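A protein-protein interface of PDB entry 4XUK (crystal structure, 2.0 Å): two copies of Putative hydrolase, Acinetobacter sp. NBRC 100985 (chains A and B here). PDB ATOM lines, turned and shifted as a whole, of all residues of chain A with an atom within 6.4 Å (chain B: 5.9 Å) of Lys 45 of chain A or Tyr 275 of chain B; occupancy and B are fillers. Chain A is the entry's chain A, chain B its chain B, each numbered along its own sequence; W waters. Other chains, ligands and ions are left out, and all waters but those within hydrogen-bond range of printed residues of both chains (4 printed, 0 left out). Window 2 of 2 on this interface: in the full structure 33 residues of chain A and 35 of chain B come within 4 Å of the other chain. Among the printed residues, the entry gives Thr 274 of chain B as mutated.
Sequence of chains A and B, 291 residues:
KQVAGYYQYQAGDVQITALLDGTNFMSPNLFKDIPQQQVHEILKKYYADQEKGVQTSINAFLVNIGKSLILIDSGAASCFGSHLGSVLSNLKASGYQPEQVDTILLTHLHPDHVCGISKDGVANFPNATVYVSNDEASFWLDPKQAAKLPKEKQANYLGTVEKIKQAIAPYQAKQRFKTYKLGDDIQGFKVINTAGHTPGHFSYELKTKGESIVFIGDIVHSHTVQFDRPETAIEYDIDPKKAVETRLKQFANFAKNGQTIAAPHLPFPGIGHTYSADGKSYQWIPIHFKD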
ATOM      1  N   HIS A  40      -0.228  -5.861 -15.800  1.00  0.00           N
ATOM      2  CA  HIS A  40       1.117  -6.421 -15.866  1.00  0.00           C
ATOM      3  C   HIS A  40       1.168  -7.792 -16.540  1.00  0.00           C
ATOM      4  O   HIS A  40       2.123  -8.093 -17.260  1.00  0.00           O
ATOM      5  CB  HIS A  40       1.800  -6.417 -14.487  1.00  0.00           C
ATOM      6  CG  HIS A  40       2.195  -5.048 -14.032  1.00  0.00           C
ATOM      7  ND1 HIS A  40       3.111  -4.277 -14.716  1.00  0.00           N
ATOM      8  CD2 HIS A  40       1.777  -4.296 -12.984  1.00  0.00           C
ATOM      9  CE1 HIS A  40       3.249  -3.114 -14.104  1.00  0.00           C
ATOM     10  NE2 HIS A  40       2.447  -3.098 -13.052  1.00  0.00           N
ATOM     11  N   GLU A  41       0.139  -8.610 -16.324  1.00  0.00           N
ATOM     12  CA  GLU A  41       0.006  -9.872 -17.056  1.00  0.00           C
ATOM     13  C   GLU A  41       0.005  -9.640 -18.569  1.00  0.00           C
ATOM     14  O   GLU A  41       0.759 -10.276 -19.312  1.00  0.00           O
ATOM     15  CB  GLU A  41      -1.285 -10.579 -16.636  1.00  0.00           C
ATOM     16  CG  GLU A  41      -1.213 -11.185 -15.232  1.00  0.00           C
ATOM     17  CD  GLU A  41      -2.589 -11.477 -14.648  1.00  0.00           C
ATOM     18  OE1 GLU A  41      -2.696 -11.659 -13.411  1.00  0.00           O
ATOM     19  OE2 GLU A  41      -3.559 -11.522 -15.433  1.00  0.00           O
ATOM     20  N   ILE A  42      -0.834  -8.717 -19.030  1.00  0.00           N
ATOM     21  CA  ILE A  42      -0.920  -8.446 -20.466  1.00  0.00           C
ATOM     22  C   ILE A  42       0.409  -7.900 -21.001  1.00  0.00           C
ATOM     23  O   ILE A  42       0.887  -8.344 -22.048  1.00  0.00           O
ATOM     24  CB  ILE A  42      -2.130  -7.543 -20.799  1.00  0.00           C
ATOM     25  CG1 ILE A  42      -3.437  -8.265 -20.441  1.00  0.00           C
ATOM     26  CG2 ILE A  42      -2.140  -7.164 -22.275  1.00  0.00           C
ATOM     27  CD1 ILE A  42      -4.661  -7.365 -20.360  1.00  0.00           C
ATOM     28  N   LEU A  43       1.027  -6.971 -20.275  1.00  0.00           N
ATOM     29  CA  LEU A  43       2.315  -6.418 -20.703  1.00  0.00           C
ATOM     30  C   LEU A  43       3.415  -7.498 -20.787  1.00  0.00           C
ATOM     31  O   LEU A  43       4.282  -7.462 -21.666  1.00  0.00           O
ATOM     32  CB  LEU A  43       2.727  -5.274 -19.769  1.00  0.00           C
ATOM     33  CG  LEU A  43       1.873  -4.007 -19.794  1.00  0.00           C
ATOM     34  CD1 LEU A  43       2.315  -3.022 -18.723  1.00  0.00           C
ATOM     35  CD2 LEU A  43       1.936  -3.354 -21.166  1.00  0.00           C
ATOM     36  N   LYS A  44       3.386  -8.457 -19.868  1.00  0.00           N
ATOM     37  CA  LYS A  44       4.373  -9.528 -19.891  1.00  0.00           C
ATOM     38  C   LYS A  44       4.192 -10.435 -21.104  1.00  0.00           C
ATOM     39  O   LYS A  44       5.174 -10.903 -21.673  1.00  0.00           O
ATOM     40  CB  LYS A  44       4.311 -10.345 -18.601  1.00  0.00           C
ATOM     41  CG  LYS A  44       4.977  -9.686 -17.409  1.00  0.00           C
ATOM     42  CD  LYS A  44       4.682 -10.479 -16.140  1.00  0.00           C
ATOM     43  CE  LYS A  44       5.598 -10.076 -14.994  1.00  0.00           C
ATOM     44  NZ  LYS A  44       4.873  -9.258 -13.976  1.00  0.00           N
ATOM     45  N   LYS A  45       2.942 -10.689 -21.497  1.00  0.00           N
ATOM     46  CA  LYS A  45       2.687 -11.489 -22.693  1.00  0.00           C
ATOM     47  C   LYS A  45       3.331 -10.833 -23.915  1.00  0.00           C
ATOM     48  O   LYS A  45       3.898 -11.517 -24.780  1.00  0.00           O
ATOM     49  CB  LYS A  45       1.179 -11.665 -22.911  1.00  0.00           C
ATOM     50  CG  LYS A  45       0.771 -11.865 -24.379  1.00  0.00           C
ATOM     51  CD  LYS A  45      -0.748 -11.920 -24.542  1.00  0.00           C
ATOM     52  CE  LYS A  45      -1.151 -11.977 -26.010  1.00  0.00           C
ATOM     53  NZ  LYS A  45      -2.629 -11.935 -26.220  1.00  0.00           N
ATOM     54  N   TYR A  46       3.263  -9.506 -23.977  1.00  0.00           N
ATOM     55  CA  TYR A  46       3.782  -8.786 -25.130  1.00  0.00           C
ATOM     56  C   TYR A  46       5.214  -8.312 -24.913  1.00  0.00           C
ATOM     57  O   TYR A  46       5.718  -7.480 -25.679  1.00  0.00           O
ATOM     58  CB  TYR A  46       2.895  -7.582 -25.450  1.00  0.00           C
ATOM     59  CG  TYR A  46       1.557  -7.916 -26.072  1.00  0.00           C
ATOM     60  CD1 TYR A  46       1.425  -8.081 -27.448  1.00  0.00           C
ATOM     61  CD2 TYR A  46       0.416  -8.029 -25.289  1.00  0.00           C
ATOM     62  CE1 TYR A  46       0.191  -8.370 -28.019  1.00  0.00           C
ATOM     63  CE2 TYR A  46      -0.810  -8.311 -25.848  1.00  0.00           C
ATOM     64  CZ  TYR A  46      -0.921  -8.477 -27.210  1.00  0.00           C
ATOM     65  OH  TYR A  46      -2.162  -8.759 -27.755  1.00  0.00           O
ATOM     66  N   TYR A  47       5.870  -8.850 -23.884  1.00  0.00           N
ATOM     67  CA  TYR A  47       7.245  -8.475 -23.565  1.00  0.00           C
ATOM     68  C   TYR A  47       7.410  -6.950 -23.542  1.00  0.00           C
ATOM     69  O   TYR A  47       8.246  -6.377 -24.246  1.00  0.00           O
ATOM     70  CB  TYR A  47       8.202  -9.151 -24.541  1.00  0.00           C
ATOM     71  CG  TYR A  47       8.252 -10.654 -24.338  1.00  0.00           C
ATOM     72  CD1 TYR A  47       7.304 -11.491 -24.918  1.00  0.00           C
ATOM     73  CD2 TYR A  47       9.232 -11.226 -23.550  1.00  0.00           C
ATOM     74  CE1 TYR A  47       7.346 -12.851 -24.731  1.00  0.00           C
ATOM     75  CE2 TYR A  47       9.287 -12.580 -23.359  1.00  0.00           C
ATOM     76  CZ  TYR A  47       8.345 -13.387 -23.950  1.00  0.00           C
ATOM     77  OH  TYR A  47       8.415 -14.747 -23.751  1.00  0.00           O
ATOM     78  N   ALA A  48       6.570  -6.313 -22.738  1.00  0.00           N
ATOM     79  CA  ALA A  48       6.444  -4.864 -22.710  1.00  0.00           C
ATOM     80  C   ALA A  48       6.317  -4.378 -21.276  1.00  0.00           C
ATOM     81  O   ALA A  48       5.821  -3.267 -21.039  1.00  0.00           O
ATOM     82  CB  ALA A  48       5.204  -4.438 -23.513  1.00  0.00           C
ATOM     83  N   ASP A 228      -6.173  -6.859 -26.029  1.00  0.00           N
ATOM     84  CA  ASP A 228      -6.646  -8.017 -25.265  1.00  0.00           C
ATOM     85  C   ASP A 228      -7.873  -7.651 -24.428  1.00  0.00           C
ATOM     86  O   ASP A 228      -8.781  -8.466 -24.263  1.00  0.00           O
ATOM     87  CB  ASP A 228      -5.535  -8.547 -24.343  1.00  0.00           C
ATOM     88  CG  ASP A 228      -4.397  -9.207 -25.101  1.00  0.00           C
ATOM     89  OD1 ASP A 228      -4.228  -8.928 -26.309  1.00  0.00           O
ATOM     90  OD2 ASP A 228      -3.653 -10.003 -24.480  1.00  0.00           O
ATOM     91  N   TYR A 282      -9.114  -8.405 -29.345  1.00  0.00           N
ATOM     92  CA  TYR A 282      -8.599  -8.082 -30.669  1.00  0.00           C
ATOM     93  C   TYR A 282      -7.097  -8.262 -30.652  1.00  0.00           C
ATOM     94  O   TYR A 282      -6.496  -8.282 -29.581  1.00  0.00           O
ATOM     95  CB  TYR A 282      -8.975  -6.648 -31.046  1.00  0.00           C
ATOM     96  CG  TYR A 282     -10.468  -6.469 -31.146  1.00  0.00           C
ATOM     97  CD1 TYR A 282     -11.125  -6.677 -32.347  1.00  0.00           C
ATOM     98  CD2 TYR A 282     -11.222  -6.127 -30.034  1.00  0.00           C
ATOM     99  CE1 TYR A 282     -12.493  -6.539 -32.443  1.00  0.00           C
ATOM    100  CE2 TYR A 282     -12.596  -5.982 -30.123  1.00  0.00           C
ATOM    101  CZ  TYR A 282     -13.219  -6.192 -31.334  1.00  0.00           C
ATOM    102  OH  TYR A 282     -14.579  -6.053 -31.443  1.00  0.00           O
ATOM    103  N   GLN A 283      -6.498  -8.413 -31.833  1.00  0.00           N
ATOM    104  CA  GLN A 283      -5.046  -8.551 -31.942  1.00  0.00           C
ATOM    105  C   GLN A 283      -4.529  -7.616 -33.037  1.00  0.00           C
ATOM    106  O   GLN A 283      -5.096  -7.562 -34.134  1.00  0.00           O
ATOM    107  CB  GLN A 283      -4.653 -10.008 -32.238  1.00  0.00           C
ATOM    108  CG  GLN A 283      -3.136 -10.234 -32.385  1.00  0.00           C
ATOM    109  CD  GLN A 283      -2.769 -11.690 -32.687  1.00  0.00           C
ATOM    110  OE1 GLN A 283      -3.539 -12.607 -32.408  1.00  0.00           O
ATOM    111  NE2 GLN A 283      -1.584 -11.900 -33.267  1.00  0.00           N
ATOM    112  N   PHE B 227       3.711 -20.487 -36.128  1.00  0.00           N
ATOM    113  CA  PHE B 227       3.552 -20.109 -34.726  1.00  0.00           C
ATOM    114  C   PHE B 227       2.213 -20.637 -34.212  1.00  0.00           C
ATOM    115  O   PHE B 227       2.163 -21.285 -33.165  1.00  0.00           O
ATOM    116  CB  PHE B 227       3.679 -18.587 -34.548  1.00  0.00           C
ATOM    117  CG  PHE B 227       5.096 -18.126 -34.356  1.00  0.00           C
ATOM    118  CD1 PHE B 227       5.980 -18.096 -35.427  1.00  0.00           C
ATOM    119  CD2 PHE B 227       5.555 -17.762 -33.099  1.00  0.00           C
ATOM    120  CE1 PHE B 227       7.298 -17.698 -35.252  1.00  0.00           C
ATOM    121  CE2 PHE B 227       6.873 -17.363 -32.913  1.00  0.00           C
ATOM    122  CZ  PHE B 227       7.745 -17.327 -33.992  1.00  0.00           C
ATOM    123  N   ALA B 255       9.469 -19.547 -25.019  1.00  0.00           N
ATOM    124  CA  ALA B 255       8.224 -19.126 -24.389  1.00  0.00           C
ATOM    125  C   ALA B 255       8.378 -19.115 -22.878  1.00  0.00           C
ATOM    126  O   ALA B 255       7.845 -18.242 -22.192  1.00  0.00           O
ATOM    127  CB  ALA B 255       7.091 -20.046 -24.802  1.00  0.00           C
ATOM    128  N   HIS B 273      10.159 -11.684 -29.443  1.00  0.00           N
ATOM    129  CA  HIS B 273      10.042 -12.720 -28.441  1.00  0.00           C
ATOM    130  C   HIS B 273       8.899 -13.662 -28.761  1.00  0.00           C
ATOM    131  O   HIS B 273       8.048 -13.339 -29.548  1.00  0.00           O
ATOM    132  CB  HIS B 273       9.779 -12.112 -27.095  1.00  0.00           C
ATOM    133  CG  HIS B 273      10.830 -11.189 -26.661  1.00  0.00           C
ATOM    134  ND1 HIS B 273      10.942  -9.926 -27.148  1.00  0.00           N
ATOM    135  CD2 HIS B 273      11.880 -11.372 -25.855  1.00  0.00           C
ATOM    136  CE1 HIS B 273      11.982  -9.349 -26.616  1.00  0.00           C
ATOM    137  NE2 HIS B 273      12.571 -10.204 -25.826  1.00  0.00           N
ATOM    138  N   THR B 274       8.900 -14.816 -28.120  1.00  0.00           N
ATOM    139  CA  THR B 274       7.885 -15.819 -28.328  1.00  0.00           C
ATOM    140  C   THR B 274       6.991 -15.927 -27.110  1.00  0.00           C
ATOM    141  O   THR B 274       7.496 -16.043 -26.046  1.00  0.00           O
ATOM    142  CB  THR B 274       8.544 -17.201 -28.558  1.00  0.00           C
ATOM    143  OG1 THR B 274       9.414 -17.134 -29.659  1.00  0.00           O
ATOM    144  CG2 THR B 274       7.589 -18.209 -28.820  1.00  0.00           C
ATOM    145  N   TYR B 275       5.677 -15.927 -27.311  1.00  0.00           N
ATOM    146  CA  TYR B 275       4.713 -16.077 -26.226  1.00  0.00           C
ATOM    147  C   TYR B 275       3.923 -17.342 -26.476  1.00  0.00           C
ATOM    148  O   TYR B 275       3.739 -17.740 -27.628  1.00  0.00           O
ATOM    149  CB  TYR B 275       3.740 -14.877 -26.221  1.00  0.00           C
ATOM    150  CG  TYR B 275       2.476 -15.123 -25.421  1.00  0.00           C
ATOM    151  CD1 TYR B 275       2.489 -15.054 -24.036  1.00  0.00           C
ATOM    152  CD2 TYR B 275       1.269 -15.425 -26.054  1.00  0.00           C
ATOM    153  CE1 TYR B 275       1.342 -15.281 -23.296  1.00  0.00           C
ATOM    154  CE2 TYR B 275       0.119 -15.653 -25.328  1.00  0.00           C
ATOM    155  CZ  TYR B 275       0.166 -15.583 -23.950  1.00  0.00           C
ATOM    156  OH  TYR B 275      -0.978 -15.811 -23.212  1.00  0.00           O
ATOM    157  N   SER B 276       3.460 -17.985 -25.408  1.00  0.00           N
ATOM    158  CA  SER B 276       2.498 -19.075 -25.552  1.00  0.00           C
ATOM    159  C   SER B 276       1.543 -19.076 -24.370  1.00  0.00           C
ATOM    160  O   SER B 276       1.960 -18.914 -23.229  1.00  0.00           O
ATOM    161  CB  SER B 276       3.202 -20.434 -25.639  1.00  0.00           C
ATOM    162  OG  SER B 276       2.230 -21.464 -25.718  1.00  0.00           O
ATOM    163  N   ALA B 277       0.263 -19.274 -24.646  1.00  0.00           N
ATOM    164  CA  ALA B 277      -0.741 -19.306 -23.594  1.00  0.00           C
ATOM    165  C   ALA B 277      -0.934 -20.704 -23.020  1.00  0.00           C
ATOM    166  O   ALA B 277      -1.433 -20.849 -21.899  1.00  0.00           O
ATOM    167  CB  ALA B 277      -2.065 -18.787 -24.124  1.00  0.00           C
ATOM    168  N   SER B 281       0.245 -23.573 -28.908  1.00  0.00           N
ATOM    169  CA  SER B 281       0.453 -22.650 -30.012  1.00  0.00           C
ATOM    170  C   SER B 281       1.339 -21.506 -29.533  1.00  0.00           C
ATOM    171  O   SER B 281       1.402 -21.223 -28.333  1.00  0.00           O
ATOM    172  CB  SER B 281      -0.882 -22.100 -30.472  1.00  0.00           C
ATOM    173  OG  SER B 281      -1.523 -21.409 -29.410  1.00  0.00           O
ATOM    174  N   TYR B 282       2.024 -20.847 -30.464  1.00  0.00           N
ATOM    175  CA  TYR B 282       2.926 -19.759 -30.103  1.00  0.00           C
ATOM    176  C   TYR B 282       2.550 -18.485 -30.834  1.00  0.00           C
ATOM    177  O   TYR B 282       1.825 -18.527 -31.834  1.00  0.00           O
ATOM    178  CB  TYR B 282       4.379 -20.153 -30.403  1.00  0.00           C
ATOM    179  CG  TYR B 282       4.822 -21.336 -29.585  1.00  0.00           C
ATOM    180  CD1 TYR B 282       4.639 -22.637 -30.043  1.00  0.00           C
ATOM    181  CD2 TYR B 282       5.411 -21.155 -28.345  1.00  0.00           C
ATOM    182  CE1 TYR B 282       5.033 -23.730 -29.277  1.00  0.00           C
ATOM    183  CE2 TYR B 282       5.811 -22.240 -27.573  1.00  0.00           C
ATOM    184  CZ  TYR B 282       5.626 -23.521 -28.046  1.00  0.00           C
ATOM    185  OH  TYR B 282       6.030 -24.596 -27.271  1.00  0.00           O
ATOM    186  N   GLN B 283       3.030 -17.350 -30.326  1.00  0.00           N
ATOM    187  CA  GLN B 283       2.761 -16.060 -30.950  1.00  0.00           C
ATOM    188  C   GLN B 283       4.069 -15.279 -31.077  1.00  0.00           C
ATOM    189  O   GLN B 283       4.867 -15.231 -30.143  1.00  0.00           O
ATOM    190  CB  GLN B 283       1.730 -15.270 -30.136  1.00  0.00           C
ATOM    191  CG  GLN B 283       1.248 -13.993 -30.816  1.00  0.00           C
ATOM    192  CD  GLN B 283       0.006 -13.405 -30.158  1.00  0.00           C
ATOM    193  OE1 GLN B 283      -0.789 -14.121 -29.548  1.00  0.00           O
ATOM    194  NE2 GLN B 283      -0.160 -12.096 -30.278  1.00  0.00           N
ATOM    195  N   TRP B 284       4.298 -14.688 -32.241  1.00  0.00           N
ATOM    196  CA  TRP B 284       5.498 -13.900 -32.453  1.00  0.00           C
ATOM    197  C   TRP B 284       5.210 -12.485 -32.003  1.00  0.00           C
ATOM    198  O   TRP B 284       4.299 -11.840 -32.527  1.00  0.00           O
ATOM    199  CB  TRP B 284       5.865 -13.922 -33.934  1.00  0.00           C
ATOM    200  CG  TRP B 284       6.947 -12.978 -34.342  1.00  0.00           C
ATOM    201  CD1 TRP B 284       6.838 -11.931 -35.221  1.00  0.00           C
ATOM    202  CD2 TRP B 284       8.313 -13.004 -33.920  1.00  0.00           C
ATOM    203  NE1 TRP B 284       8.053 -11.306 -35.365  1.00  0.00           N
ATOM    204  CE2 TRP B 284       8.976 -11.950 -34.579  1.00  0.00           C
ATOM    205  CE3 TRP B 284       9.043 -13.828 -33.062  1.00  0.00           C
ATOM    206  CZ2 TRP B 284      10.328 -11.686 -34.386  1.00  0.00           C
ATOM    207  CZ3 TRP B 284      10.377 -13.566 -32.874  1.00  0.00           C
ATOM    208  CH2 TRP B 284      11.011 -12.508 -33.538  1.00  0.00           C
ATOM    209  N   ILE B 285       5.982 -12.017 -31.024  1.00  0.00           N
ATOM    210  CA  ILE B 285       5.845 -10.655 -30.519  1.00  0.00           C
ATOM    211  C   ILE B 285       7.018  -9.825 -31.023  1.00  0.00           C
ATOM    212  O   ILE B 285       8.121  -9.900 -30.483  1.00  0.00           O
ATOM    213  CB  ILE B 285       5.807 -10.615 -28.970  1.00  0.00           C
ATOM    214  CG1 ILE B 285       4.837 -11.665 -28.414  1.00  0.00           C
ATOM    215  CG2 ILE B 285       5.429  -9.212 -28.479  1.00  0.00           C
ATOM    216  CD1 ILE B 285       3.368 -11.459 -28.845  1.00  0.00           C
HETATM  217  O   HOH W   1       8.150 -15.304 -20.965  1.00  0.00           O
HETATM  218  O   HOH W   2      -2.284 -15.112 -32.036  1.00  0.00           O
HETATM  219  O   HOH W   3      -3.107 -13.737 -28.401  1.00  0.00           O
HETATM  220  O   HOH W   4      -2.701 -11.360 -29.234  1.00  0.00           O
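Along chain B the printed residues that touch a printed residue of chain A span positions 255 to 285.
Hydrophobic or aromatic side chains of chain A that line the printed part of chain B: Tyr 47.
Among the printed residues, 7 pairs touch across the chains.
Among the printed residues, no Asp or Glu carboxylate lies within 4 Å of a Lys or Arg side-chain nitrogen of the other chain.
The side-chain amino group of Lys 45 of chain A lies within salt-bridge range of the side-chain carboxylate of Asp 228 of chain A (2.8 Å).
The side-chain carboxylate (OD1) of Asp 228 of chain A lies within hydrogen-bond range of the side-chain hydroxyl (OH) of Tyr 46 of chain A (2.5 Å).
The backbone carbonyl oxygen (O) of His 273 of chain B lies within hydrogen-bond range of the backbone NH (N) of Ile 285 of chain B, at 2.9 Å.
The backbone NH of Gln 283 of chain B lies within hydrogen-bond range of the backbone carbonyl oxygen of Tyr 275 of chain B (2.8 Å).
CE1 of Tyr 275 of chain B touches CG of Lys 45 of chain A, 3.6 Å away.
O of Lys 45 of chain A touches CG1 of Ile 285 of chain B (3.8 Å).
Tyr 46 of chain A touches Ile 285 of chain B (O to CG2, 3.3 Å).
OH of Tyr 47 of chain A touches O of Ala 255 of chain B (3.9 Å).
CD1 of Tyr 47 of chain A touches CB of His 273 of chain B, 3.4 Å away.
Lys 44 of chain A touches none of the printed residues of chain B.
Of the printed residues of chain B, Tyr 46 of chain A touches Ile 285 (3.3 Å).
Of the printed residues of chain A, His 273 of chain B touches Tyr 47 (3.4 Å).
Of chain A, only Lys 45 (3.6 Å) comes within 4 Å of Tyr 275 of chain B.
Trp 284 of chain B touches none of the printed residues of chain A.
The nearest printed residue of chain B that does not touch Gln 283 of chain A is Trp 284 of chain B (5.9 Å).
Gln 283 of chain B touches its own counterpart, Gln 283 of chain A.
Positions printed for both chains: 282 and 283.
Of the 7 pairs that touch across the chains among the printed residues, 1 has its exchanged pair printed and touching as well.
The side-chain hydroxyl (OH) of Tyr 47 of chain A sits at hydrogen-bond distance from the backbone carbonyl oxygen (O) of Thr 274 of chain B (2.8 Å).
The side-chain amide nitrogen of Gln 283 of chain B sits close to the side-chain amide nitrogen of Gln 283 of chain A (3.3 Å).
Water W3 bridges OE1 of Gln 283 of chain B and NZ of Lys 45 of chain A.
Water W2 lies within hydrogen-bond range of OE1 of Gln 283 of chain A (2.8 Å) and OE1 of Gln 283 of chain B (3.1 Å).
Water W4 lies within hydrogen-bond range of NE2 of Gln 283 of chain B (2.8 Å), OH of Tyr 46 of chain A (3.0 Å) and NZ of Lys 45 of chain A (3.1 Å).
Water W1 lies within hydrogen-bond range of OH of Tyr 47 of chain A (2.9 Å) and O of Ala 255 of chain B (3.2 Å).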
